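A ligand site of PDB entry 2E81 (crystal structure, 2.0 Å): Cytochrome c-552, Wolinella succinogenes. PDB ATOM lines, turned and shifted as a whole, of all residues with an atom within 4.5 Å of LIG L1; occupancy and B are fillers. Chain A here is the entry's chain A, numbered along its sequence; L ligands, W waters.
Water W1 lies within hydrogen-bond range of O of Ala 376 (2.6 Å), OH of Tyr 74 (2.6 Å), O4 of LIG L1 (2.7 Å) and NE2 of His 378 (3.2 Å). Water W4 lies within hydrogen-bond range of O4 of LIG L1 (2.7 Å), OD1 of Asp 257 (2.8 Å) and N of His 378 (3.0 Å). Water W3 bridges O2 of LIG L1 (2.8 Å) and O1 of LG2 L2 (3.3 Å). Water W7 lies within hydrogen-bond range of O1 of LIG L1 and OD1 of Asn 75. Water W5 lies within hydrogen-bond range of the side-chain hydroxyl of Thr 90, an oxygen (O1) of LIG L1, the guanidinium group of Arg 92, the backbone NH of Tyr 74 and the side-chain amide oxygen of Asn 75. Water W8 lies within hydrogen-bond range of NE2 of His 378, O of Asn 75, O3 of LIG L1 and OH of Tyr 74.
ND2 of Asn 87 lies within hydrogen-bond range of O of Cys 108 (3.3 Å). The backbone carbonyl oxygen (O) of Asn 87 is in hydrogen-bond range of the side-chain hydroxyl (OG1) of Thr 93 (3.1 Å). NE2 of His 378 sits at hydrogen-bond distance from OH of Tyr 74 (2.9 Å). SG of Cys 111 is in hydrogen-bond range of OH of Tyr 163, 3.3 Å away. A ring nitrogen (ND1) of His 193 lies within hydrogen-bond range of the side-chain carboxylate (OD2) of Asp 257, at 2.7 Å. The side-chain hydroxyl (OH) of Tyr 163 is in hydrogen-bond range of the backbone carbonyl oxygen (O) of Gln 191, 2.6 Å away. The side-chain hydroxyl (OG1) of Thr 93 lies within hydrogen-bond range of the backbone carbonyl oxygen (O) of Thr 90 (3.0 Å). The backbone NH (N) of Arg 92 lies close to the side-chain hydroxyl (OG1) of Thr 90.
A nitrogen (N1) of LG2 L2 is bound to an iron atom (FE1) of LIG L1 (1.7 Å).
SG of Cys 192 is covalently linked to C25 of LG3 L3, at 1.8 Å. The side-chain amino group of Lys 112 is bound to an iron atom (FE1) of LIG L1, 2.1 Å away. SG of Cys 108 is bonded to C18 of LIG L1, 1.8 Å away. An iron atom (FE1) of LG3 L3 is bound by a ring nitrogen (NE2) of His 193. The side-chain carboxylate (OD2) of Asp 86 lies close to an oxygen (O4) of LG3 L3 (2.5 Å). N1 of LG2 L2 lies close to NE2 of His 255 (3.2 Å). An oxygen (O1) of LIG L1 sits at hydrogen-bond distance from the backbone NH (N) of Asn 75 (2.9 Å). The guanidinium group (NH1) of Arg 92 lies within salt-bridge range of an oxygen (O2) of LIG L1 (3.0 Å). The guanidinium group (NH2) of Arg 92 is in hydrogen-bond range of an oxygen (O1) of LG2 L2 (3.0 Å). The side-chain sulfur of Cys 111 is covalently linked to a carbon (C25) of LIG L1 (1.8 Å).
A ring nitrogen (NE2) of His 255 lies close to a nitrogen (N4) of LIG L1 (3.5 Å). Tyr 74 touches LIG L1. Pro 77 touches LIG L1 (CB to C33, 3.9 Å). Asp 86 touches LIG L1 (O to C9, 3.3 Å). Asn 87 touches LIG L1 (ND2 to C2, 3.4 Å). Thr 90 touches LIG L1. Thr 93 touches LIG L1. Leu 104 touches LIG L1. OH of Tyr 163 touches C26 of LIG L1, at 3.8 Å. Gln 191 touches LIG L1 (O to C26, 3.9 Å). Cys 192 touches LIG L1 (O to C25, 3.5 Å). ND1 of His 193 touches C31 of LIG L1, 3.4 Å away. Tyr 196 touches LIG L1 (OH to C3, 3.2 Å). CE2 of Phe 198 touches C19 of LIG L1, at 3.8 Å. Val 216 touches LIG L1 (CG2 to C24, 3.9 Å). O of Ala 376 touches O4 of LIG L1 (3.5 Å). His 378 touches LIG L1 (CD2 to O4, 3.3 Å). Of the 26 residues printed, 22 come within 4 Å of LIG L1.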
ATOM      1  N   TYR A  74      -4.121 -19.271   4.939  1.00  0.00           N
ATOM      2  CA  TYR A  74      -3.901 -20.632   5.432  1.00  0.00           C
ATOM      3  C   TYR A  74      -3.737 -20.559   6.944  1.00  0.00           C
ATOM      4  O   TYR A  74      -2.743 -20.018   7.431  1.00  0.00           O
ATOM      5  CB  TYR A  74      -2.654 -21.263   4.808  1.00  0.00           C
ATOM      6  CG  TYR A  74      -2.271 -22.592   5.436  1.00  0.00           C
ATOM      7  CD1 TYR A  74      -3.141 -23.683   5.399  1.00  0.00           C
ATOM      8  CD2 TYR A  74      -1.045 -22.757   6.084  1.00  0.00           C
ATOM      9  CE1 TYR A  74      -2.802 -24.912   5.989  1.00  0.00           C
ATOM     10  CE2 TYR A  74      -0.688 -23.969   6.671  1.00  0.00           C
ATOM     11  CZ  TYR A  74      -1.571 -25.041   6.624  1.00  0.00           C
ATOM     12  OH  TYR A  74      -1.218 -26.238   7.205  1.00  0.00           O
ATOM     13  N   ASN A  75      -4.705 -21.102   7.675  1.00  0.00           N
ATOM     14  CA  ASN A  75      -4.640 -21.075   9.127  1.00  0.00           C
ATOM     15  C   ASN A  75      -4.598 -22.499   9.695  1.00  0.00           C
ATOM     16  O   ASN A  75      -4.888 -23.468   8.985  1.00  0.00           O
ATOM     17  CB  ASN A  75      -5.868 -20.351   9.693  1.00  0.00           C
ATOM     18  CG  ASN A  75      -6.148 -19.032   8.983  1.00  0.00           C
ATOM     19  OD1 ASN A  75      -7.278 -18.777   8.555  1.00  0.00           O
ATOM     20  ND2 ASN A  75      -5.127 -18.189   8.876  1.00  0.00           N
ATOM     21  N   ALA A  76      -4.247 -22.618  10.972  1.00  0.00           N
ATOM     22  CA  ALA A  76      -4.192 -23.913  11.620  1.00  0.00           C
ATOM     23  C   ALA A  76      -5.645 -24.364  11.777  1.00  0.00           C
ATOM     24  O   ALA A  76      -6.555 -23.539  11.735  1.00  0.00           O
ATOM     25  CB  ALA A  76      -3.537 -23.804  12.977  1.00  0.00           C
ATOM     26  N   PRO A  77      -5.877 -25.670  11.950  1.00  0.00           N
ATOM     27  CA  PRO A  77      -7.263 -26.091  12.104  1.00  0.00           C
ATOM     28  C   PRO A  77      -7.789 -25.779  13.488  1.00  0.00           C
ATOM     29  O   PRO A  77      -7.028 -25.625  14.437  1.00  0.00           O
ATOM     30  CB  PRO A  77      -7.201 -27.588  11.828  1.00  0.00           C
ATOM     31  CG  PRO A  77      -5.865 -27.969  12.371  1.00  0.00           C
ATOM     32  CD  PRO A  77      -4.965 -26.829  11.923  1.00  0.00           C
ATOM     33  N   ASP A  86     -15.343 -21.739   8.244  1.00  0.00           N
ATOM     34  CA  ASP A  86     -13.963 -21.439   7.850  1.00  0.00           C
ATOM     35  C   ASP A  86     -13.786 -21.675   6.359  1.00  0.00           C
ATOM     36  O   ASP A  86     -12.980 -21.021   5.704  1.00  0.00           O
ATOM     37  CB  ASP A  86     -12.980 -22.278   8.675  1.00  0.00           C
ATOM     38  CG  ASP A  86     -12.865 -21.800  10.106  1.00  0.00           C
ATOM     39  OD1 ASP A  86     -13.201 -20.609  10.361  1.00  0.00           O
ATOM     40  OD2 ASP A  86     -12.444 -22.585  10.977  1.00  0.00           O
ATOM     41  N   ASN A  87     -14.568 -22.618   5.822  1.00  0.00           N
ATOM     42  CA  ASN A  87     -14.542 -22.940   4.406  1.00  0.00           C
ATOM     43  C   ASN A  87     -15.049 -21.706   3.663  1.00  0.00           C
ATOM     44  O   ASN A  87     -14.530 -21.340   2.607  1.00  0.00           O
ATOM     45  CB  ASN A  87     -15.463 -24.137   4.138  1.00  0.00           C
ATOM     46  CG  ASN A  87     -15.381 -24.656   2.723  1.00  0.00           C
ATOM     47  OD1 ASN A  87     -16.401 -24.816   2.038  1.00  0.00           O
ATOM     48  ND2 ASN A  87     -14.162 -24.936   2.262  1.00  0.00           N
ATOM     49  N   THR A  90     -12.301 -18.444   4.490  1.00  0.00           N
ATOM     50  CA  THR A  90     -10.976 -18.456   3.892  1.00  0.00           C
ATOM     51  C   THR A  90     -10.938 -17.677   2.583  1.00  0.00           C
ATOM     52  O   THR A  90     -11.855 -17.761   1.769  1.00  0.00           O
ATOM     53  CB  THR A  90     -10.449 -19.888   3.638  1.00  0.00           C
ATOM     54  OG1 THR A  90      -9.116 -19.806   3.132  1.00  0.00           O
ATOM     55  CG2 THR A  90     -11.328 -20.641   2.637  1.00  0.00           C
ATOM     56  N   ARG A  92      -9.197 -18.322   0.237  1.00  0.00           N
ATOM     57  CA  ARG A  92      -9.014 -19.274  -0.855  1.00  0.00           C
ATOM     58  C   ARG A  92     -10.282 -19.491  -1.680  1.00  0.00           C
ATOM     59  O   ARG A  92     -10.199 -19.688  -2.891  1.00  0.00           O
ATOM     60  CB  ARG A  92      -8.479 -20.616  -0.319  1.00  0.00           C
ATOM     61  CG  ARG A  92      -7.177 -20.496   0.470  1.00  0.00           C
ATOM     62  CD  ARG A  92      -6.331 -21.781   0.459  1.00  0.00           C
ATOM     63  NE  ARG A  92      -6.999 -22.942   1.034  1.00  0.00           N
ATOM     64  CZ  ARG A  92      -7.046 -23.219   2.335  1.00  0.00           C
ATOM     65  NH1 ARG A  92      -6.457 -22.410   3.210  1.00  0.00           N
ATOM     66  NH2 ARG A  92      -7.681 -24.306   2.760  1.00  0.00           N
ATOM     67  N   THR A  93     -11.457 -19.458  -1.050  1.00  0.00           N
ATOM     68  CA  THR A  93     -12.698 -19.648  -1.792  1.00  0.00           C
ATOM     69  C   THR A  93     -13.156 -18.375  -2.516  1.00  0.00           C
ATOM     70  O   THR A  93     -14.130 -18.391  -3.260  1.00  0.00           O
ATOM     71  CB  THR A  93     -13.839 -20.156  -0.882  1.00  0.00           C
ATOM     72  OG1 THR A  93     -13.865 -19.381   0.324  1.00  0.00           O
ATOM     73  CG2 THR A  93     -13.651 -21.634  -0.570  1.00  0.00           C
ATOM     74  N   LEU A 104     -12.968 -21.607  -6.738  1.00  0.00           N
ATOM     75  CA  LEU A 104     -12.966 -23.041  -6.462  1.00  0.00           C
ATOM     76  C   LEU A 104     -14.232 -23.819  -6.829  1.00  0.00           C
ATOM     77  O   LEU A 104     -15.315 -23.250  -6.955  1.00  0.00           O
ATOM     78  CB  LEU A 104     -12.600 -23.268  -4.986  1.00  0.00           C
ATOM     79  CG  LEU A 104     -11.249 -22.623  -4.620  1.00  0.00           C
ATOM     80  CD1 LEU A 104     -10.895 -22.914  -3.159  1.00  0.00           C
ATOM     81  CD2 LEU A 104     -10.159 -23.165  -5.541  1.00  0.00           C
ATOM     82  N   ALA A 107     -16.287 -29.434  -5.013  1.00  0.00           N
ATOM     83  CA  ALA A 107     -15.599 -30.407  -4.176  1.00  0.00           C
ATOM     84  C   ALA A 107     -15.054 -29.848  -2.863  1.00  0.00           C
ATOM     85  O   ALA A 107     -14.761 -30.602  -1.941  1.00  0.00           O
ATOM     86  CB  ALA A 107     -14.469 -31.080  -4.969  1.00  0.00           C
ATOM     87  N   CYS A 108     -14.923 -28.526  -2.777  1.00  0.00           N
ATOM     88  CA  CYS A 108     -14.415 -27.916  -1.551  1.00  0.00           C
ATOM     89  C   CYS A 108     -15.332 -28.049  -0.344  1.00  0.00           C
ATOM     90  O   CYS A 108     -14.901 -27.810   0.789  1.00  0.00           O
ATOM     91  CB  CYS A 108     -14.065 -26.452  -1.780  1.00  0.00           C
ATOM     92  SG  CYS A 108     -12.485 -26.217  -2.632  1.00  0.00           S
ATOM     93  N   THR A 110     -17.008 -30.962   0.323  1.00  0.00           N
ATOM     94  CA  THR A 110     -16.894 -32.368   0.668  1.00  0.00           C
ATOM     95  C   THR A 110     -16.595 -32.785   2.096  1.00  0.00           C
ATOM     96  O   THR A 110     -17.311 -33.610   2.667  1.00  0.00           O
ATOM     97  CB  THR A 110     -15.874 -33.074  -0.254  1.00  0.00           C
ATOM     98  OG1 THR A 110     -16.166 -32.728  -1.617  1.00  0.00           O
ATOM     99  CG2 THR A 110     -15.987 -34.592  -0.106  1.00  0.00           C
ATOM    100  N   CYS A 111     -15.544 -32.232   2.688  1.00  0.00           N
ATOM    101  CA  CYS A 111     -15.157 -32.626   4.036  1.00  0.00           C
ATOM    102  C   CYS A 111     -15.496 -31.581   5.079  1.00  0.00           C
ATOM    103  O   CYS A 111     -14.786 -31.444   6.080  1.00  0.00           O
ATOM    104  CB  CYS A 111     -13.659 -32.930   4.046  1.00  0.00           C
ATOM    105  SG  CYS A 111     -13.129 -34.102   2.750  1.00  0.00           S
ATOM    106  N   LYS A 112     -16.586 -30.852   4.870  1.00  0.00           N
ATOM    107  CA  LYS A 112     -16.965 -29.803   5.803  1.00  0.00           C
ATOM    108  C   LYS A 112     -18.384 -29.908   6.334  1.00  0.00           C
ATOM    109  O   LYS A 112     -18.738 -29.216   7.282  1.00  0.00           O
ATOM    110  CB  LYS A 112     -16.831 -28.432   5.113  1.00  0.00           C
ATOM    111  CG  LYS A 112     -15.450 -28.133   4.518  1.00  0.00           C
ATOM    112  CD  LYS A 112     -14.399 -28.032   5.623  1.00  0.00           C
ATOM    113  CE  LYS A 112     -13.040 -27.627   5.067  1.00  0.00           C
ATOM    114  NZ  LYS A 112     -12.342 -28.706   4.312  1.00  0.00           N
ATOM    115  N   TYR A 163     -15.099 -42.126  -2.228  1.00  0.00           N
ATOM    116  CA  TYR A 163     -13.678 -42.045  -2.577  1.00  0.00           C
ATOM    117  C   TYR A 163     -12.736 -42.715  -1.579  1.00  0.00           C
ATOM    118  O   TYR A 163     -11.611 -43.076  -1.936  1.00  0.00           O
ATOM    119  CB  TYR A 163     -13.261 -40.580  -2.803  1.00  0.00           C
ATOM    120  CG  TYR A 163     -13.448 -39.657  -1.621  1.00  0.00           C
ATOM    121  CD1 TYR A 163     -12.593 -39.723  -0.520  1.00  0.00           C
ATOM    122  CD2 TYR A 163     -14.456 -38.699  -1.614  1.00  0.00           C
ATOM    123  CE1 TYR A 163     -12.748 -38.848   0.560  1.00  0.00           C
ATOM    124  CE2 TYR A 163     -14.620 -37.829  -0.543  1.00  0.00           C
ATOM    125  CZ  TYR A 163     -13.759 -37.906   0.539  1.00  0.00           C
ATOM    126  OH  TYR A 163     -13.927 -37.050   1.610  1.00  0.00           O
ATOM    127  N   GLN A 191     -12.080 -40.142   6.215  1.00  0.00           N
ATOM    128  CA  GLN A 191     -12.941 -39.661   5.142  1.00  0.00           C
ATOM    129  C   GLN A 191     -12.454 -38.260   4.771  1.00  0.00           C
ATOM    130  O   GLN A 191     -12.559 -37.847   3.615  1.00  0.00           O
ATOM    131  CB  GLN A 191     -14.387 -39.514   5.619  1.00  0.00           C
ATOM    132  CG  GLN A 191     -15.034 -40.769   6.136  1.00  0.00           C
ATOM    133  CD  GLN A 191     -16.446 -40.477   6.604  1.00  0.00           C
ATOM    134  OE1 GLN A 191     -17.351 -40.290   5.791  1.00  0.00           O
ATOM    135  NE2 GLN A 191     -16.630 -40.403   7.909  1.00  0.00           N
ATOM    136  N   CYS A 192     -11.918 -37.553   5.748  1.00  0.00           N
ATOM    137  CA  CYS A 192     -11.470 -36.186   5.539  1.00  0.00           C
ATOM    138  C   CYS A 192     -10.008 -35.912   5.825  1.00  0.00           C
ATOM    139  O   CYS A 192      -9.362 -35.134   5.127  1.00  0.00           O
ATOM    140  CB  CYS A 192     -12.327 -35.241   6.383  1.00  0.00           C
ATOM    141  SG  CYS A 192     -14.113 -35.518   6.233  1.00  0.00           S
ATOM    142  N   HIS A 193      -9.485 -36.530   6.879  1.00  0.00           N
ATOM    143  CA  HIS A 193      -8.104 -36.317   7.277  1.00  0.00           C
ATOM    144  C   HIS A 193      -7.093 -37.108   6.469  1.00  0.00           C
ATOM    145  O   HIS A 193      -6.322 -37.900   7.015  1.00  0.00           O
ATOM    146  CB  HIS A 193      -7.971 -36.608   8.775  1.00  0.00           C
ATOM    147  CG  HIS A 193      -8.584 -35.561   9.647  1.00  0.00           C
ATOM    148  ND1 HIS A 193      -7.929 -34.414  10.069  1.00  0.00           N
ATOM    149  CD2 HIS A 193      -9.848 -35.458  10.143  1.00  0.00           C
ATOM    150  CE1 HIS A 193      -8.801 -33.684  10.781  1.00  0.00           C
ATOM    151  NE2 HIS A 193      -9.977 -34.269  10.866  1.00  0.00           N
ATOM    152  N   TYR A 196      -5.361 -35.621  -0.844  1.00  0.00           N
ATOM    153  CA  TYR A 196      -6.215 -35.873  -2.003  1.00  0.00           C
ATOM    154  C   TYR A 196      -5.874 -34.894  -3.125  1.00  0.00           C
ATOM    155  O   TYR A 196      -5.072 -33.980  -2.953  1.00  0.00           O
ATOM    156  CB  TYR A 196      -7.672 -35.625  -1.613  1.00  0.00           C
ATOM    157  CG  TYR A 196      -7.944 -34.136  -1.458  1.00  0.00           C
ATOM    158  CD1 TYR A 196      -7.555 -33.447  -0.295  1.00  0.00           C
ATOM    159  CD2 TYR A 196      -8.482 -33.392  -2.497  1.00  0.00           C
ATOM    160  CE1 TYR A 196      -7.680 -32.055  -0.200  1.00  0.00           C
ATOM    161  CE2 TYR A 196      -8.616 -32.006  -2.413  1.00  0.00           C
ATOM    162  CZ  TYR A 196      -8.212 -31.347  -1.277  1.00  0.00           C
ATOM    163  OH  TYR A 196      -8.313 -29.974  -1.223  1.00  0.00           O
ATOM    164  N   PHE A 198      -8.005 -33.255  -6.990  1.00  0.00           N
ATOM    165  CA  PHE A 198      -9.232 -33.265  -7.772  1.00  0.00           C
ATOM    166  C   PHE A 198      -8.946 -33.812  -9.155  1.00  0.00           C
ATOM    167  O   PHE A 198      -8.099 -33.281  -9.877  1.00  0.00           O
ATOM    168  CB  PHE A 198      -9.826 -31.858  -7.911  1.00  0.00           C
ATOM    169  CG  PHE A 198     -10.261 -31.225  -6.620  1.00  0.00           C
ATOM    170  CD1 PHE A 198     -10.788 -32.000  -5.583  1.00  0.00           C
ATOM    171  CD2 PHE A 198     -10.197 -29.844  -6.449  1.00  0.00           C
ATOM    172  CE1 PHE A 198     -11.240 -31.415  -4.412  1.00  0.00           C
ATOM    173  CE2 PHE A 198     -10.654 -29.244  -5.283  1.00  0.00           C
ATOM    174  CZ  PHE A 198     -11.175 -30.029  -4.264  1.00  0.00           C
ATOM    175  N   VAL A 216     -12.917 -35.785  -5.933  1.00  0.00           N
ATOM    176  CA  VAL A 216     -11.937 -36.000  -4.876  1.00  0.00           C
ATOM    177  C   VAL A 216     -11.368 -37.388  -5.068  1.00  0.00           C
ATOM    178  O   VAL A 216     -12.130 -38.368  -5.148  1.00  0.00           O
ATOM    179  CB  VAL A 216     -12.591 -35.905  -3.474  1.00  0.00           C
ATOM    180  CG1 VAL A 216     -11.627 -36.399  -2.411  1.00  0.00           C
ATOM    181  CG2 VAL A 216     -12.980 -34.464  -3.192  1.00  0.00           C
ATOM    182  N   HIS A 255      -3.165 -32.043   4.529  1.00  0.00           N
ATOM    183  CA  HIS A 255      -3.439 -32.828   5.730  1.00  0.00           C
ATOM    184  C   HIS A 255      -3.493 -34.353   5.570  1.00  0.00           C
ATOM    185  O   HIS A 255      -4.574 -34.948   5.640  1.00  0.00           O
ATOM    186  CB  HIS A 255      -4.743 -32.329   6.344  1.00  0.00           C
ATOM    187  CG  HIS A 255      -5.814 -32.096   5.325  1.00  0.00           C
ATOM    188  ND1 HIS A 255      -6.310 -33.101   4.519  1.00  0.00           N
ATOM    189  CD2 HIS A 255      -6.444 -30.957   4.941  1.00  0.00           C
ATOM    190  CE1 HIS A 255      -7.195 -32.587   3.669  1.00  0.00           C
ATOM    191  NE2 HIS A 255      -7.290 -31.291   3.912  1.00  0.00           N
ATOM    192  N   ASP A 257      -3.148 -36.646   7.437  1.00  0.00           N
ATOM    193  CA  ASP A 257      -3.147 -37.088   8.830  1.00  0.00           C
ATOM    194  C   ASP A 257      -3.167 -38.606   8.998  1.00  0.00           C
ATOM    195  O   ASP A 257      -2.344 -39.169   9.726  1.00  0.00           O
ATOM    196  CB  ASP A 257      -4.333 -36.476   9.582  1.00  0.00           C
ATOM    197  CG  ASP A 257      -4.408 -34.956   9.422  1.00  0.00           C
ATOM    198  OD1 ASP A 257      -3.421 -34.269   9.745  1.00  0.00           O
ATOM    199  OD2 ASP A 257      -5.462 -34.453   8.965  1.00  0.00           O
ATOM    200  N   ALA A 376       2.038 -30.776   6.551  1.00  0.00           N
ATOM    201  CA  ALA A 376       0.643 -30.491   6.253  1.00  0.00           C
ATOM    202  C   ALA A 376      -0.293 -31.125   7.279  1.00  0.00           C
ATOM    203  O   ALA A 376      -1.404 -30.645   7.508  1.00  0.00           O
ATOM    204  CB  ALA A 376       0.285 -30.977   4.851  1.00  0.00           C
ATOM    205  N   HIS A 378      -0.803 -31.393  10.833  1.00  0.00           N
ATOM    206  CA  HIS A 378      -0.345 -30.722  12.058  1.00  0.00           C
ATOM    207  C   HIS A 378      -0.031 -31.619  13.243  1.00  0.00           C
ATOM    208  O   HIS A 378       0.666 -31.207  14.174  1.00  0.00           O
ATOM    209  CB  HIS A 378      -1.367 -29.661  12.464  1.00  0.00           C
ATOM    210  CG  HIS A 378      -1.490 -28.541  11.479  1.00  0.00           C
ATOM    211  ND1 HIS A 378      -0.626 -27.478  11.435  1.00  0.00           N
ATOM    212  CD2 HIS A 378      -2.369 -28.349  10.458  1.00  0.00           C
ATOM    213  CE1 HIS A 378      -0.952 -26.673  10.442  1.00  0.00           C
ATOM    214  NE2 HIS A 378      -2.016 -27.178   9.835  1.00  0.00           N
HETATM  215  C1  LIG L   1      -9.289 -27.617   6.873  1.00  0.00           C
HETATM  216  C2  LIG L   1     -10.871 -25.240   3.001  1.00  0.00           C
HETATM  217  C3  LIG L   1     -10.934 -29.372   0.508  1.00  0.00           C
HETATM  218  C4  LIG L   1     -10.372 -31.728   4.663  1.00  0.00           C
HETATM  219  C5  LIG L   1      -9.741 -26.586   6.054  1.00  0.00           C
HETATM  220  C6  LIG L   1      -9.767 -25.167   6.422  1.00  0.00           C
HETATM  221  C7  LIG L   1     -10.253 -24.512   5.336  1.00  0.00           C
HETATM  222  C8  LIG L   1     -10.488 -25.508   4.313  1.00  0.00           C
HETATM  223  C9  LIG L   1     -10.448 -23.004   5.185  1.00  0.00           C
HETATM  224  C10 LIG L   1      -9.276 -24.531   7.729  1.00  0.00           C
HETATM  225  C11 LIG L   1      -7.744 -24.484   7.788  1.00  0.00           C
HETATM  226  C12 LIG L   1      -7.151 -23.559   6.752  1.00  0.00           C
HETATM  227  O1  LIG L   1      -7.199 -22.318   6.955  1.00  0.00           O
HETATM  228  O2  LIG L   1      -6.657 -24.057   5.719  1.00  0.00           O
HETATM  229  C13 LIG L   1     -11.008 -26.150   1.967  1.00  0.00           C
HETATM  230  C14 LIG L   1     -11.191 -25.782   0.580  1.00  0.00           C
HETATM  231  C15 LIG L   1     -11.139 -26.932  -0.150  1.00  0.00           C
HETATM  232  C16 LIG L   1     -10.943 -28.002   0.807  1.00  0.00           C
HETATM  233  C17 LIG L   1     -11.372 -24.386   0.025  1.00  0.00           C
HETATM  234  C18 LIG L   1     -11.241 -27.023  -1.534  1.00  0.00           C
HETATM  235  C19 LIG L   1     -10.067 -26.917  -2.301  1.00  0.00           C
HETATM  236  C20 LIG L   1     -10.791 -30.406   1.429  1.00  0.00           C
HETATM  237  C21 LIG L   1     -11.083 -31.795   1.155  1.00  0.00           C
HETATM  238  C22 LIG L   1     -11.009 -32.464   2.337  1.00  0.00           C
HETATM  239  C23 LIG L   1     -10.633 -31.464   3.329  1.00  0.00           C
HETATM  240  C24 LIG L   1     -11.455 -32.393  -0.214  1.00  0.00           C
HETATM  241  C25 LIG L   1     -11.324 -33.805   2.570  1.00  0.00           C
HETATM  242  C26 LIG L   1     -10.822 -34.876   1.775  1.00  0.00           C
HETATM  243  C27 LIG L   1      -9.972 -30.821   5.615  1.00  0.00           C
HETATM  244  C28 LIG L   1      -9.426 -31.181   6.910  1.00  0.00           C
HETATM  245  C29 LIG L   1      -8.938 -30.043   7.469  1.00  0.00           C
HETATM  246  C30 LIG L   1      -9.293 -28.955   6.546  1.00  0.00           C
HETATM  247  C31 LIG L   1      -9.384 -32.562   7.555  1.00  0.00           C
HETATM  248  C32 LIG L   1      -8.284 -29.963   8.832  1.00  0.00           C
HETATM  249  C33 LIG L   1      -6.818 -30.328   9.074  1.00  0.00           C
HETATM  250  C34 LIG L   1      -5.848 -29.319   8.487  1.00  0.00           C
HETATM  251  O3  LIG L   1      -6.300 -28.243   8.047  1.00  0.00           O
HETATM  252  O4  LIG L   1      -4.636 -29.599   8.465  1.00  0.00           O
HETATM  253  N1  LIG L   1     -10.187 -26.773   4.765  1.00  0.00           N
HETATM  254  N2  LIG L   1     -10.827 -27.498   2.102  1.00  0.00           N
HETATM  255  N3  LIG L   1     -10.549 -30.207   2.776  1.00  0.00           N
HETATM  256  N4  LIG L   1      -9.854 -29.453   5.384  1.00  0.00           N
HETATM  257 FE1  LIG L   1     -10.304 -28.474   3.726  1.00  0.00          FE
HETATM  258  N1  LG2 L   2      -8.660 -28.420   3.294  1.00  0.00           N
HETATM  259  O1  LG2 L   2      -7.958 -27.250   2.978  1.00  0.00           O
HETATM  260  C1  LG3 L   3     -10.262 -30.359  12.509  1.00  0.00           C
HETATM  261  C2  LG3 L   3      -9.605 -34.727  14.358  1.00  0.00           C
HETATM  262  C3  LG3 L   3     -13.121 -36.465  11.673  1.00  0.00           C
HETATM  263  C4  LG3 L   3     -12.890 -32.464   9.058  1.00  0.00           C
HETATM  264  C5  LG3 L   3      -9.953 -31.359  13.412  1.00  0.00           C
HETATM  265  C6  LG3 L   3      -9.047 -31.216  14.536  1.00  0.00           C
HETATM  266  C7  LG3 L   3      -8.818 -32.463  15.009  1.00  0.00           C
HETATM  267  C8  LG3 L   3      -9.588 -33.364  14.197  1.00  0.00           C
HETATM  268  C9  LG3 L   3      -7.950 -32.855  16.198  1.00  0.00           C
HETATM  269  C10 LG3 L   3      -8.551 -29.918  15.180  1.00  0.00           C
HETATM  270  C11 LG3 L   3      -9.388 -29.582  16.414  1.00  0.00           C
HETATM  271  C12 LG3 L   3      -8.942 -28.303  17.081  1.00  0.00           C
HETATM  272  O1  LG3 L   3      -8.064 -27.605  16.523  1.00  0.00           O
HETATM  273  O2  LG3 L   3      -9.473 -27.968  18.165  1.00  0.00           O
HETATM  274  C13 LG3 L   3     -10.465 -35.612  13.756  1.00  0.00           C
HETATM  275  C14 LG3 L   3     -10.639 -36.993  14.152  1.00  0.00           C
HETATM  276  C15 LG3 L   3     -11.725 -37.464  13.514  1.00  0.00           C
HETATM  277  C16 LG3 L   3     -12.168 -36.371  12.663  1.00  0.00           C
HETATM  278  C17 LG3 L   3      -9.729 -37.776  15.099  1.00  0.00           C
HETATM  279  C18 LG3 L   3     -12.274 -38.751  13.643  1.00  0.00           C
HETATM  280  C19 LG3 L   3     -12.870 -39.176  14.859  1.00  0.00           C
HETATM  281  C20 LG3 L   3     -13.410 -35.497  10.731  1.00  0.00           C
HETATM  282  C21 LG3 L   3     -14.280 -35.711   9.606  1.00  0.00           C
HETATM  283  C22 LG3 L   3     -14.156 -34.621   8.808  1.00  0.00           C
HETATM  284  C23 LG3 L   3     -13.237 -33.727   9.486  1.00  0.00           C
HETATM  285  C24 LG3 L   3     -15.123 -36.945   9.291  1.00  0.00           C
HETATM  286  C25 LG3 L   3     -14.755 -34.456   7.555  1.00  0.00           C
HETATM  287  C26 LG3 L   3     -16.153 -34.430   7.372  1.00  0.00           C
HETATM  288  C27 LG3 L   3     -12.124 -31.534   9.746  1.00  0.00           C
HETATM  289  C28 LG3 L   3     -12.032 -30.129   9.397  1.00  0.00           C
HETATM  290  C29 LG3 L   3     -11.279 -29.532  10.351  1.00  0.00           C
HETATM  291  C30 LG3 L   3     -10.950 -30.556  11.320  1.00  0.00           C
HETATM  292  C31 LG3 L   3     -12.647 -29.457   8.180  1.00  0.00           C
HETATM  293  C32 LG3 L   3     -10.895 -28.061  10.350  1.00  0.00           C
HETATM  294  C33 LG3 L   3     -11.859 -27.280  11.225  1.00  0.00           C
HETATM  295  C34 LG3 L   3     -11.692 -25.780  11.071  1.00  0.00           C
HETATM  296  O3  LG3 L   3     -10.537 -25.301  11.162  1.00  0.00           O
HETATM  297  O4  LG3 L   3     -12.711 -25.087  10.882  1.00  0.00           O
HETATM  298  N1  LG3 L   3     -10.322 -32.692  13.242  1.00  0.00           N
HETATM  299  N2  LG3 L   3     -11.403 -35.227  12.842  1.00  0.00           N
HETATM  300  N3  LG3 L   3     -12.784 -34.267  10.667  1.00  0.00           N
HETATM  301  N4  LG3 L   3     -11.504 -31.784  10.948  1.00  0.00           N
HETATM  302 FE1  LG3 L   3     -11.514 -33.479  11.932  1.00  0.00          FE
HETATM  303  O   HOH W   1      -2.665 -28.444   6.995  1.00  0.00           O
HETATM  304  O   HOH W   2      -7.925 -25.881   0.430  1.00  0.00           O
HETATM  305  O   HOH W   3      -5.937 -26.734   5.515  1.00  0.00           O
HETATM  306  O   HOH W   4      -3.719 -31.517  10.192  1.00  0.00           O
HETATM  307  O   HOH W   5      -7.465 -20.012   5.295  1.00  0.00           O
HETATM  308  O   HOH W   6     -13.808 -29.916   2.006  1.00  0.00           O
HETATM  309  O   HOH W   7      -9.284 -21.141   8.475  1.00  0.00           O
HETATM  310  O   HOH W   8      -4.295 -26.206   8.620  1.00  0.00           O
